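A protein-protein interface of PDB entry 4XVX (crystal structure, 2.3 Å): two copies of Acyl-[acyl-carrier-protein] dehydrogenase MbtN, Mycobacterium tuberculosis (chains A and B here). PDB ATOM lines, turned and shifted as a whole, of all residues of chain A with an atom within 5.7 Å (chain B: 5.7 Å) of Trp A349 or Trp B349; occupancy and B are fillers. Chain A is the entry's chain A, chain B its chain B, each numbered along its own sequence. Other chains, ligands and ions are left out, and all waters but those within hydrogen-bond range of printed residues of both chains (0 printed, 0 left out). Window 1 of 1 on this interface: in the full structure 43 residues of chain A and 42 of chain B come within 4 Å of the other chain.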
ATOM      1  N   VAL A 201      -4.081  -5.903  28.751  1.00  0.00           N
ATOM      2  CA  VAL A 201      -5.183  -4.920  28.778  1.00  0.00           C
ATOM      3  C   VAL A 201      -4.953  -3.856  29.895  1.00  0.00           C
ATOM      4  O   VAL A 201      -5.127  -2.665  29.676  1.00  0.00           O
ATOM      5  CB  VAL A 201      -6.553  -5.634  28.865  1.00  0.00           C
ATOM      6  CG1 VAL A 201      -7.694  -4.655  29.160  1.00  0.00           C
ATOM      7  CG2 VAL A 201      -6.825  -6.440  27.594  1.00  0.00           C
ATOM      8  N   GLU A 323     -15.824  -4.946  39.388  1.00  0.00           N
ATOM      9  CA  GLU A 323     -16.030  -4.610  37.988  1.00  0.00           C
ATOM     10  C   GLU A 323     -17.134  -3.548  37.852  1.00  0.00           C
ATOM     11  O   GLU A 323     -16.920  -2.529  37.197  1.00  0.00           O
ATOM     12  CB  GLU A 323     -16.379  -5.845  37.182  1.00  0.00           C
ATOM     13  CG  GLU A 323     -16.439  -5.573  35.687  1.00  0.00           C
ATOM     14  CD  GLU A 323     -16.831  -6.754  34.822  1.00  0.00           C
ATOM     15  OE1 GLU A 323     -17.716  -7.536  35.235  1.00  0.00           O
ATOM     16  OE2 GLU A 323     -16.311  -6.855  33.692  1.00  0.00           O
ATOM     17  N   ILE A 326     -16.111   0.044  39.481  1.00  0.00           N
ATOM     18  CA  ILE A 326     -15.203   0.826  38.644  1.00  0.00           C
ATOM     19  C   ILE A 326     -15.876   1.310  37.340  1.00  0.00           C
ATOM     20  O   ILE A 326     -15.653   2.454  36.943  1.00  0.00           O
ATOM     21  CB  ILE A 326     -13.840   0.119  38.398  1.00  0.00           C
ATOM     22  CG1 ILE A 326     -13.226  -0.371  39.749  1.00  0.00           C
ATOM     23  CG2 ILE A 326     -12.869   1.092  37.692  1.00  0.00           C
ATOM     24  CD1 ILE A 326     -13.042   0.733  40.916  1.00  0.00           C
ATOM     25  N   SER A 327     -16.714   0.469  36.722  1.00  0.00           N
ATOM     26  CA  SER A 327     -17.439   0.807  35.499  1.00  0.00           C
ATOM     27  C   SER A 327     -18.368   1.986  35.740  1.00  0.00           C
ATOM     28  O   SER A 327     -18.465   2.871  34.881  1.00  0.00           O
ATOM     29  CB  SER A 327     -18.256  -0.394  35.016  1.00  0.00           C
ATOM     30  OG  SER A 327     -19.171  -0.004  34.004  1.00  0.00           O
ATOM     31  N   MET A 330     -16.320   5.234  36.456  1.00  0.00           N
ATOM     32  CA  MET A 330     -15.813   5.705  35.161  1.00  0.00           C
ATOM     33  C   MET A 330     -16.924   6.391  34.371  1.00  0.00           C
ATOM     34  O   MET A 330     -16.665   7.431  33.791  1.00  0.00           O
ATOM     35  CB  MET A 330     -15.170   4.565  34.354  1.00  0.00           C
ATOM     36  CG  MET A 330     -14.411   5.057  33.153  1.00  0.00           C
ATOM     37  SD  MET A 330     -13.800   3.706  32.149  1.00  0.00           S
ATOM     38  CE  MET A 330     -13.355   4.606  30.636  1.00  0.00           C
ATOM     39  N   THR A 344      -7.429   9.069  35.430  1.00  0.00           N
ATOM     40  CA  THR A 344      -6.833   7.726  35.465  1.00  0.00           C
ATOM     41  C   THR A 344      -7.900   6.625  35.616  1.00  0.00           C
ATOM     42  O   THR A 344      -7.545   5.457  35.792  1.00  0.00           O
ATOM     43  CB  THR A 344      -5.746   7.640  36.550  1.00  0.00           C
ATOM     44  OG1 THR A 344      -6.340   7.988  37.783  1.00  0.00           O
ATOM     45  CG2 THR A 344      -4.582   8.578  36.289  1.00  0.00           C
ATOM     46  N   LEU A 345      -9.192   6.991  35.470  1.00  0.00           N
ATOM     47  CA  LEU A 345     -10.309   6.063  35.565  1.00  0.00           C
ATOM     48  C   LEU A 345     -10.218   4.891  34.622  1.00  0.00           C
ATOM     49  O   LEU A 345     -10.620   3.798  35.016  1.00  0.00           O
ATOM     50  CB  LEU A 345     -11.672   6.766  35.388  1.00  0.00           C
ATOM     51  CG  LEU A 345     -12.333   7.347  36.615  1.00  0.00           C
ATOM     52  CD1 LEU A 345     -12.859   6.253  37.552  1.00  0.00           C
ATOM     53  CD2 LEU A 345     -11.438   8.398  37.294  1.00  0.00           C
ATOM     54  N   GLY A 346      -9.728   5.122  33.395  1.00  0.00           N
ATOM     55  CA  GLY A 346      -9.574   4.059  32.411  1.00  0.00           C
ATOM     56  C   GLY A 346      -8.599   2.994  32.887  1.00  0.00           C
ATOM     57  O   GLY A 346      -8.851   1.792  32.729  1.00  0.00           O
ATOM     58  N   LYS A 347      -7.474   3.434  33.491  1.00  0.00           N
ATOM     59  CA  LYS A 347      -6.452   2.551  34.047  1.00  0.00           C
ATOM     60  C   LYS A 347      -7.058   1.661  35.148  1.00  0.00           C
ATOM     61  O   LYS A 347      -6.860   0.438  35.136  1.00  0.00           O
ATOM     62  CB  LYS A 347      -5.257   3.375  34.576  1.00  0.00           C
ATOM     63  CG  LYS A 347      -4.040   2.540  34.961  1.00  0.00           C
ATOM     64  CD  LYS A 347      -2.708   3.265  34.721  1.00  0.00           C
ATOM     65  CE  LYS A 347      -2.446   4.424  35.656  1.00  0.00           C
ATOM     66  NZ  LYS A 347      -2.215   5.677  34.891  1.00  0.00           N
ATOM     67  N   TRP A 348      -7.850   2.267  36.058  1.00  0.00           N
ATOM     68  CA  TRP A 348      -8.519   1.531  37.137  1.00  0.00           C
ATOM     69  C   TRP A 348      -9.439   0.469  36.578  1.00  0.00           C
ATOM     70  O   TRP A 348      -9.403  -0.692  37.006  1.00  0.00           O
ATOM     71  CB  TRP A 348      -9.367   2.490  37.950  1.00  0.00           C
ATOM     72  CG  TRP A 348      -8.607   3.492  38.754  1.00  0.00           C
ATOM     73  CD1 TRP A 348      -7.253   3.580  38.919  1.00  0.00           C
ATOM     74  CD2 TRP A 348      -9.182   4.526  39.548  1.00  0.00           C
ATOM     75  NE1 TRP A 348      -6.949   4.637  39.746  1.00  0.00           N
ATOM     76  CE2 TRP A 348      -8.117   5.231  40.153  1.00  0.00           C
ATOM     77  CE3 TRP A 348     -10.503   4.944  39.798  1.00  0.00           C
ATOM     78  CZ2 TRP A 348      -8.336   6.314  41.003  1.00  0.00           C
ATOM     79  CZ3 TRP A 348     -10.713   6.054  40.595  1.00  0.00           C
ATOM     80  CH2 TRP A 348      -9.638   6.729  41.186  1.00  0.00           C
ATOM     81  N   TRP A 349     -10.225   0.869  35.571  1.00  0.00           N
ATOM     82  CA  TRP A 349     -11.217   0.062  34.895  1.00  0.00           C
ATOM     83  C   TRP A 349     -10.557  -1.106  34.174  1.00  0.00           C
ATOM     84  O   TRP A 349     -10.933  -2.252  34.439  1.00  0.00           O
ATOM     85  CB  TRP A 349     -12.084   0.982  34.012  1.00  0.00           C
ATOM     86  CG  TRP A 349     -13.125   0.288  33.200  1.00  0.00           C
ATOM     87  CD1 TRP A 349     -14.282  -0.285  33.646  1.00  0.00           C
ATOM     88  CD2 TRP A 349     -13.124   0.148  31.780  1.00  0.00           C
ATOM     89  NE1 TRP A 349     -14.981  -0.817  32.590  1.00  0.00           N
ATOM     90  CE2 TRP A 349     -14.298  -0.557  31.428  1.00  0.00           C
ATOM     91  CE3 TRP A 349     -12.209   0.498  30.770  1.00  0.00           C
ATOM     92  CZ2 TRP A 349     -14.584  -0.920  30.106  1.00  0.00           C
ATOM     93  CZ3 TRP A 349     -12.482   0.116  29.462  1.00  0.00           C
ATOM     94  CH2 TRP A 349     -13.636  -0.622  29.151  1.00  0.00           C
ATOM     95  N   ARG A 350      -9.479  -0.839  33.419  1.00  0.00           N
ATOM     96  CA  ARG A 350      -8.676  -1.863  32.742  1.00  0.00           C
ATOM     97  C   ARG A 350      -8.013  -2.855  33.747  1.00  0.00           C
ATOM     98  O   ARG A 350      -7.956  -4.053  33.467  1.00  0.00           O
ATOM     99  CB  ARG A 350      -7.597  -1.220  31.804  1.00  0.00           C
ATOM    100  CG  ARG A 350      -8.116  -0.614  30.480  1.00  0.00           C
ATOM    101  CD  ARG A 350      -7.170   0.447  29.877  1.00  0.00           C
ATOM    102  NE  ARG A 350      -5.774   0.012  29.894  1.00  0.00           N
ATOM    103  CZ  ARG A 350      -4.757   0.706  30.409  1.00  0.00           C
ATOM    104  NH1 ARG A 350      -4.944   1.936  30.868  1.00  0.00           N
ATOM    105  NH2 ARG A 350      -3.535   0.186  30.432  1.00  0.00           N
ATOM    106  N   ASP A 351      -7.516  -2.362  34.899  1.00  0.00           N
ATOM    107  CA  ASP A 351      -6.897  -3.184  35.967  1.00  0.00           C
ATOM    108  C   ASP A 351      -7.941  -4.117  36.576  1.00  0.00           C
ATOM    109  O   ASP A 351      -7.700  -5.320  36.725  1.00  0.00           O
ATOM    110  CB  ASP A 351      -6.362  -2.280  37.111  1.00  0.00           C
ATOM    111  CG  ASP A 351      -5.019  -1.640  36.873  1.00  0.00           C
ATOM    112  OD1 ASP A 351      -4.506  -1.741  35.739  1.00  0.00           O
ATOM    113  OD2 ASP A 351      -4.478  -1.044  37.817  1.00  0.00           O
ATOM    114  N   MET A 352      -9.091  -3.543  36.981  1.00  0.00           N
ATOM    115  CA  MET A 352     -10.180  -4.292  37.620  1.00  0.00           C
ATOM    116  C   MET A 352     -10.698  -5.454  36.735  1.00  0.00           C
ATOM    117  O   MET A 352     -11.038  -6.480  37.282  1.00  0.00           O
ATOM    118  CB  MET A 352     -11.324  -3.338  38.040  1.00  0.00           C
ATOM    119  CG  MET A 352     -12.409  -3.998  38.896  1.00  0.00           C
ATOM    120  SD  MET A 352     -11.779  -4.652  40.486  1.00  0.00           S
ATOM    121  CE  MET A 352     -11.702  -3.196  41.451  1.00  0.00           C
ATOM    122  N   LYS A 353     -10.693  -5.324  35.379  1.00  0.00           N
ATOM    123  CA  LYS A 353     -11.153  -6.394  34.484  1.00  0.00           C
ATOM    124  C   LYS A 353     -10.377  -7.735  34.673  1.00  0.00           C
ATOM    125  O   LYS A 353     -10.932  -8.811  34.398  1.00  0.00           O
ATOM    126  CB  LYS A 353     -11.163  -5.932  33.016  1.00  0.00           C
ATOM    127  CG  LYS A 353     -11.888  -6.869  32.020  1.00  0.00           C
ATOM    128  CD  LYS A 353     -13.307  -7.220  32.468  1.00  0.00           C
ATOM    129  CE  LYS A 353     -14.142  -7.816  31.366  1.00  0.00           C
ATOM    130  NZ  LYS A 353     -15.236  -8.668  31.914  1.00  0.00           N
ATOM    131  N   VAL B 201      -9.187   6.187  26.019  1.00  0.00           N
ATOM    132  CA  VAL B 201      -9.263   4.837  26.583  1.00  0.00           C
ATOM    133  C   VAL B 201      -9.414   3.799  25.457  1.00  0.00           C
ATOM    134  O   VAL B 201      -8.787   2.750  25.497  1.00  0.00           O
ATOM    135  CB  VAL B 201     -10.377   4.755  27.663  1.00  0.00           C
ATOM    136  CG1 VAL B 201     -10.719   3.313  28.009  1.00  0.00           C
ATOM    137  CG2 VAL B 201      -9.994   5.560  28.899  1.00  0.00           C
ATOM    138  N   GLU B 323     -22.252  -2.990  26.414  1.00  0.00           N
ATOM    139  CA  GLU B 323     -21.208  -3.063  27.444  1.00  0.00           C
ATOM    140  C   GLU B 323     -21.193  -4.460  28.095  1.00  0.00           C
ATOM    141  O   GLU B 323     -20.132  -5.046  28.277  1.00  0.00           O
ATOM    142  CB  GLU B 323     -21.399  -1.969  28.491  1.00  0.00           C
ATOM    143  CG  GLU B 323     -20.304  -1.925  29.536  1.00  0.00           C
ATOM    144  CD  GLU B 323     -20.542  -0.940  30.662  1.00  0.00           C
ATOM    145  OE1 GLU B 323     -21.708  -0.789  31.090  1.00  0.00           O
ATOM    146  OE2 GLU B 323     -19.544  -0.383  31.174  1.00  0.00           O
ATOM    147  N   ILE B 326     -19.904  -7.299  25.394  1.00  0.00           N
ATOM    148  CA  ILE B 326     -18.444  -7.312  25.198  1.00  0.00           C
ATOM    149  C   ILE B 326     -17.699  -7.748  26.479  1.00  0.00           C
ATOM    150  O   ILE B 326     -16.778  -8.565  26.395  1.00  0.00           O
ATOM    151  CB  ILE B 326     -17.915  -6.002  24.601  1.00  0.00           C
ATOM    152  CG1 ILE B 326     -18.718  -5.575  23.346  1.00  0.00           C
ATOM    153  CG2 ILE B 326     -16.476  -6.168  24.252  1.00  0.00           C
ATOM    154  CD1 ILE B 326     -18.814  -6.667  22.119  1.00  0.00           C
ATOM    155  N   SER B 327     -18.167  -7.309  27.647  1.00  0.00           N
ATOM    156  CA  SER B 327     -17.551  -7.727  28.914  1.00  0.00           C
ATOM    157  C   SER B 327     -17.638  -9.256  29.131  1.00  0.00           C
ATOM    158  O   SER B 327     -16.671  -9.865  29.567  1.00  0.00           O
ATOM    159  CB  SER B 327     -18.159  -6.956  30.090  1.00  0.00           C
ATOM    160  OG  SER B 327     -17.882  -7.593  31.326  1.00  0.00           O
ATOM    161  N   MET B 330     -15.408 -11.051  26.542  1.00  0.00           N
ATOM    162  CA  MET B 330     -14.038 -10.910  27.002  1.00  0.00           C
ATOM    163  C   MET B 330     -13.725 -11.919  28.119  1.00  0.00           C
ATOM    164  O   MET B 330     -12.675 -12.576  28.075  1.00  0.00           O
ATOM    165  CB  MET B 330     -13.724  -9.478  27.437  1.00  0.00           C
ATOM    166  CG  MET B 330     -12.250  -9.268  27.751  1.00  0.00           C
ATOM    167  SD  MET B 330     -11.973  -7.543  28.159  1.00  0.00           S
ATOM    168  CE  MET B 330     -10.242  -7.598  28.663  1.00  0.00           C
ATOM    169  N   THR B 344      -8.008  -9.454  20.373  1.00  0.00           N
ATOM    170  CA  THR B 344      -8.402  -8.042  20.267  1.00  0.00           C
ATOM    171  C   THR B 344      -9.646  -7.739  21.150  1.00  0.00           C
ATOM    172  O   THR B 344     -10.203  -6.656  21.063  1.00  0.00           O
ATOM    173  CB  THR B 344      -8.589  -7.644  18.797  1.00  0.00           C
ATOM    174  OG1 THR B 344      -9.639  -8.440  18.250  1.00  0.00           O
ATOM    175  CG2 THR B 344      -7.282  -7.800  17.963  1.00  0.00           C
ATOM    176  N   LEU B 345     -10.068  -8.680  22.001  1.00  0.00           N
ATOM    177  CA  LEU B 345     -11.220  -8.517  22.926  1.00  0.00           C
ATOM    178  C   LEU B 345     -11.128  -7.254  23.812  1.00  0.00           C
ATOM    179  O   LEU B 345     -12.131  -6.592  24.029  1.00  0.00           O
ATOM    180  CB  LEU B 345     -11.398  -9.770  23.814  1.00  0.00           C
ATOM    181  CG  LEU B 345     -12.256 -10.942  23.288  1.00  0.00           C
ATOM    182  CD1 LEU B 345     -13.747 -10.623  23.318  1.00  0.00           C
ATOM    183  CD2 LEU B 345     -11.782 -11.448  21.919  1.00  0.00           C
ATOM    184  N   GLY B 346      -9.928  -6.935  24.287  1.00  0.00           N
ATOM    185  CA  GLY B 346      -9.672  -5.752  25.097  1.00  0.00           C
ATOM    186  C   GLY B 346      -9.955  -4.468  24.345  1.00  0.00           C
ATOM    187  O   GLY B 346     -10.565  -3.542  24.898  1.00  0.00           O
ATOM    188  N   LYS B 347      -9.573  -4.434  23.054  1.00  0.00           N
ATOM    189  CA  LYS B 347      -9.821  -3.285  22.176  1.00  0.00           C
ATOM    190  C   LYS B 347     -11.340  -3.092  22.009  1.00  0.00           C
ATOM    191  O   LYS B 347     -11.832  -1.966  22.176  1.00  0.00           O
ATOM    192  CB  LYS B 347      -9.110  -3.480  20.827  1.00  0.00           C
ATOM    193  CG  LYS B 347      -9.176  -2.270  19.910  1.00  0.00           C
ATOM    194  CD  LYS B 347      -7.972  -2.196  18.951  1.00  0.00           C
ATOM    195  CE  LYS B 347      -7.970  -3.226  17.829  1.00  0.00           C
ATOM    196  NZ  LYS B 347      -9.196  -3.164  16.990  1.00  0.00           N
ATOM    197  N   TRP B 348     -12.073  -4.196  21.754  1.00  0.00           N
ATOM    198  CA  TRP B 348     -13.542  -4.197  21.621  1.00  0.00           C
ATOM    199  C   TRP B 348     -14.217  -3.668  22.870  1.00  0.00           C
ATOM    200  O   TRP B 348     -15.131  -2.839  22.807  1.00  0.00           O
ATOM    201  CB  TRP B 348     -14.061  -5.615  21.396  1.00  0.00           C
ATOM    202  CG  TRP B 348     -13.695  -6.232  20.090  1.00  0.00           C
ATOM    203  CD1 TRP B 348     -13.045  -5.645  19.036  1.00  0.00           C
ATOM    204  CD2 TRP B 348     -14.010  -7.561  19.679  1.00  0.00           C
ATOM    205  NE1 TRP B 348     -12.912  -6.545  18.003  1.00  0.00           N
ATOM    206  CE2 TRP B 348     -13.491  -7.734  18.378  1.00  0.00           C
ATOM    207  CE3 TRP B 348     -14.649  -8.644  20.307  1.00  0.00           C
ATOM    208  CZ2 TRP B 348     -13.621  -8.936  17.682  1.00  0.00           C
ATOM    209  CZ3 TRP B 348     -14.756  -9.843  19.624  1.00  0.00           C
ATOM    210  CH2 TRP B 348     -14.226  -9.989  18.339  1.00  0.00           C
ATOM    211  N   TRP B 349     -13.737  -4.155  24.014  1.00  0.00           N
ATOM    212  CA  TRP B 349     -14.234  -3.799  25.328  1.00  0.00           C
ATOM    213  C   TRP B 349     -13.979  -2.311  25.616  1.00  0.00           C
ATOM    214  O   TRP B 349     -14.942  -1.601  25.894  1.00  0.00           O
ATOM    215  CB  TRP B 349     -13.625  -4.768  26.341  1.00  0.00           C
ATOM    216  CG  TRP B 349     -14.004  -4.523  27.756  1.00  0.00           C
ATOM    217  CD1 TRP B 349     -15.207  -4.791  28.350  1.00  0.00           C
ATOM    218  CD2 TRP B 349     -13.125  -4.087  28.799  1.00  0.00           C
ATOM    219  NE1 TRP B 349     -15.148  -4.479  29.686  1.00  0.00           N
ATOM    220  CE2 TRP B 349     -13.870  -4.078  29.999  1.00  0.00           C
ATOM    221  CE3 TRP B 349     -11.767  -3.712  28.836  1.00  0.00           C
ATOM    222  CZ2 TRP B 349     -13.324  -3.640  31.209  1.00  0.00           C
ATOM    223  CZ3 TRP B 349     -11.236  -3.266  30.036  1.00  0.00           C
ATOM    224  CH2 TRP B 349     -12.020  -3.198  31.193  1.00  0.00           C
ATOM    225  N   ARG B 350     -12.741  -1.818  25.371  1.00  0.00           N
ATOM    226  CA  ARG B 350     -12.357  -0.407  25.551  1.00  0.00           C
ATOM    227  C   ARG B 350     -13.176   0.538  24.621  1.00  0.00           C
ATOM    228  O   ARG B 350     -13.569   1.625  25.047  1.00  0.00           O
ATOM    229  CB  ARG B 350     -10.830  -0.203  25.330  1.00  0.00           C
ATOM    230  CG  ARG B 350      -9.903  -0.729  26.465  1.00  0.00           C
ATOM    231  CD  ARG B 350      -8.446  -0.991  26.022  1.00  0.00           C
ATOM    232  NE  ARG B 350      -7.928   0.093  25.180  1.00  0.00           N
ATOM    233  CZ  ARG B 350      -7.413  -0.058  23.961  1.00  0.00           C
ATOM    234  NH1 ARG B 350      -7.225  -1.272  23.454  1.00  0.00           N
ATOM    235  NH2 ARG B 350      -7.041   1.002  23.256  1.00  0.00           N
ATOM    236  N   ASP B 351     -13.451   0.101  23.373  1.00  0.00           N
ATOM    237  CA  ASP B 351     -14.248   0.808  22.367  1.00  0.00           C
ATOM    238  C   ASP B 351     -15.683   0.933  22.824  1.00  0.00           C
ATOM    239  O   ASP B 351     -16.239   2.032  22.809  1.00  0.00           O
ATOM    240  CB  ASP B 351     -14.213   0.035  21.031  1.00  0.00           C
ATOM    241  CG  ASP B 351     -12.993   0.319  20.138  1.00  0.00           C
ATOM    242  OD1 ASP B 351     -12.047   0.969  20.610  1.00  0.00           O
ATOM    243  OD2 ASP B 351     -13.009  -0.090  18.958  1.00  0.00           O
ATOM    244  N   MET B 352     -16.283  -0.198  23.237  1.00  0.00           N
ATOM    245  CA  MET B 352     -17.653  -0.243  23.708  1.00  0.00           C
ATOM    246  C   MET B 352     -17.935   0.664  24.948  1.00  0.00           C
ATOM    247  O   MET B 352     -19.010   1.220  25.023  1.00  0.00           O
ATOM    248  CB  MET B 352     -18.076  -1.699  23.963  1.00  0.00           C
ATOM    249  CG  MET B 352     -19.588  -1.874  24.187  1.00  0.00           C
ATOM    250  SD  MET B 352     -20.675  -1.360  22.820  1.00  0.00           S
ATOM    251  CE  MET B 352     -20.519  -2.749  21.741  1.00  0.00           C
ATOM    252  N   LYS B 353     -16.961   0.893  25.836  1.00  0.00           N
ATOM    253  CA  LYS B 353     -17.136   1.738  27.022  1.00  0.00           C
ATOM    254  C   LYS B 353     -17.528   3.199  26.681  1.00  0.00           C
ATOM    255  O   LYS B 353     -18.154   3.892  27.502  1.00  0.00           O
ATOM    256  CB  LYS B 353     -15.889   1.670  27.927  1.00  0.00           C
ATOM    257  CG  LYS B 353     -16.054   2.236  29.339  1.00  0.00           C
ATOM    258  CD  LYS B 353     -17.301   1.721  30.051  1.00  0.00           C
ATOM    259  CE  LYS B 353     -17.339   2.108  31.502  1.00  0.00           C
ATOM    260  NZ  LYS B 353     -18.753   2.158  31.983  1.00  0.00           N
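CA of Gly B346 touches CG2 of Val A201, at 3.8 Å.
Trp B349 touches Val A201 (CZ3 to CG1, 3.9 Å).
CE of Met A330 touches CG2 of Val B201, at 3.9 Å.
CA of Gly A346 touches CG2 of Val B201, at 3.8 Å.
Val B201 touches Trp A349 (CG1 to CZ3, 3.9 Å).
Trp A349 touches Trp B349.
Trp A349 touches Arg B350 (CH2 to CA, 3.8 Å).
Lys B353 touches Trp A349.
CA of Arg A350 touches CH2 of Trp B349, 3.9 Å away.
CE of Met B330 touches CG of Lys A353, 3.8 Å away.
Val A201 touches Trp B349, and with the chains exchanged Trp A349 touches Val B201.
Met A330 touches Lys B353, and with the chains exchanged Lys A353 touches Met B330.
Trp A349 touches its own counterpart, Trp B349.
Trp A349 touches Lys B353, and with the chains exchanged Lys A353 touches Trp B349.
15 positions are printed for both chains.
The side-chain hydroxyl of Ser B327 sits at hydrogen-bond distance from the side-chain carboxylate of Glu A323, 2.9 Å away.
OE2 of Glu B323 lies within hydrogen-bond range of OG of Ser A327, 2.9 Å away.
The side-chain amino group (NZ) of Lys B353 lies within hydrogen-bond range of the side-chain hydroxyl (OG) of Ser A327.
The side-chain hydroxyl of Ser B327 lies within hydrogen-bond range of the side-chain amino group of Lys A353.
O of Val B201 is in hydrogen-bond range of NE of Arg B350 (2.8 Å).
O of Val A201 is in hydrogen-bond range of NE of Arg A350, 2.8 Å away.
OE2 of Glu B323 lies within salt-bridge range of NZ of Lys B353 (2.8 Å).
NZ of Lys A353 is in salt-bridge range of OE2 of Glu A323 (2.8 Å).
Hydrophobic or aromatic side chains of chain A that line the printed part of chain B: Val A201, Met A330 and Trp A349.
Along chain A the printed residues that touch a printed residue of chain B span positions 201 to 353.
Among the printed residues, 17 pairs touch across the chains.
Trp B349 touches just these residues of chain A: Val A201, Trp A349, Arg A350 and Lys A353.
Of the printed residues of chain A, Glu B323 touches Ser A327.
Of the printed residues of chain B, Lys A353 touches Ser B327 (2.9 Å), Met B330 (3.8 Å) and Trp B349 (3.4 Å).
Of the printed residues of chain B, Arg A350 touches Trp B349 (3.9 Å).
Of the printed residues of chain B, Met A330 touches Val B201 and Lys B353.
Asp A351 touches none of the printed residues of chain B.
The nearest residue of chain B that does not touch Trp A349 is Glu B323 (4.8 Å).
The nearest residue of chain A that does not touch Trp B349 is Glu A323 (4.8 Å).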
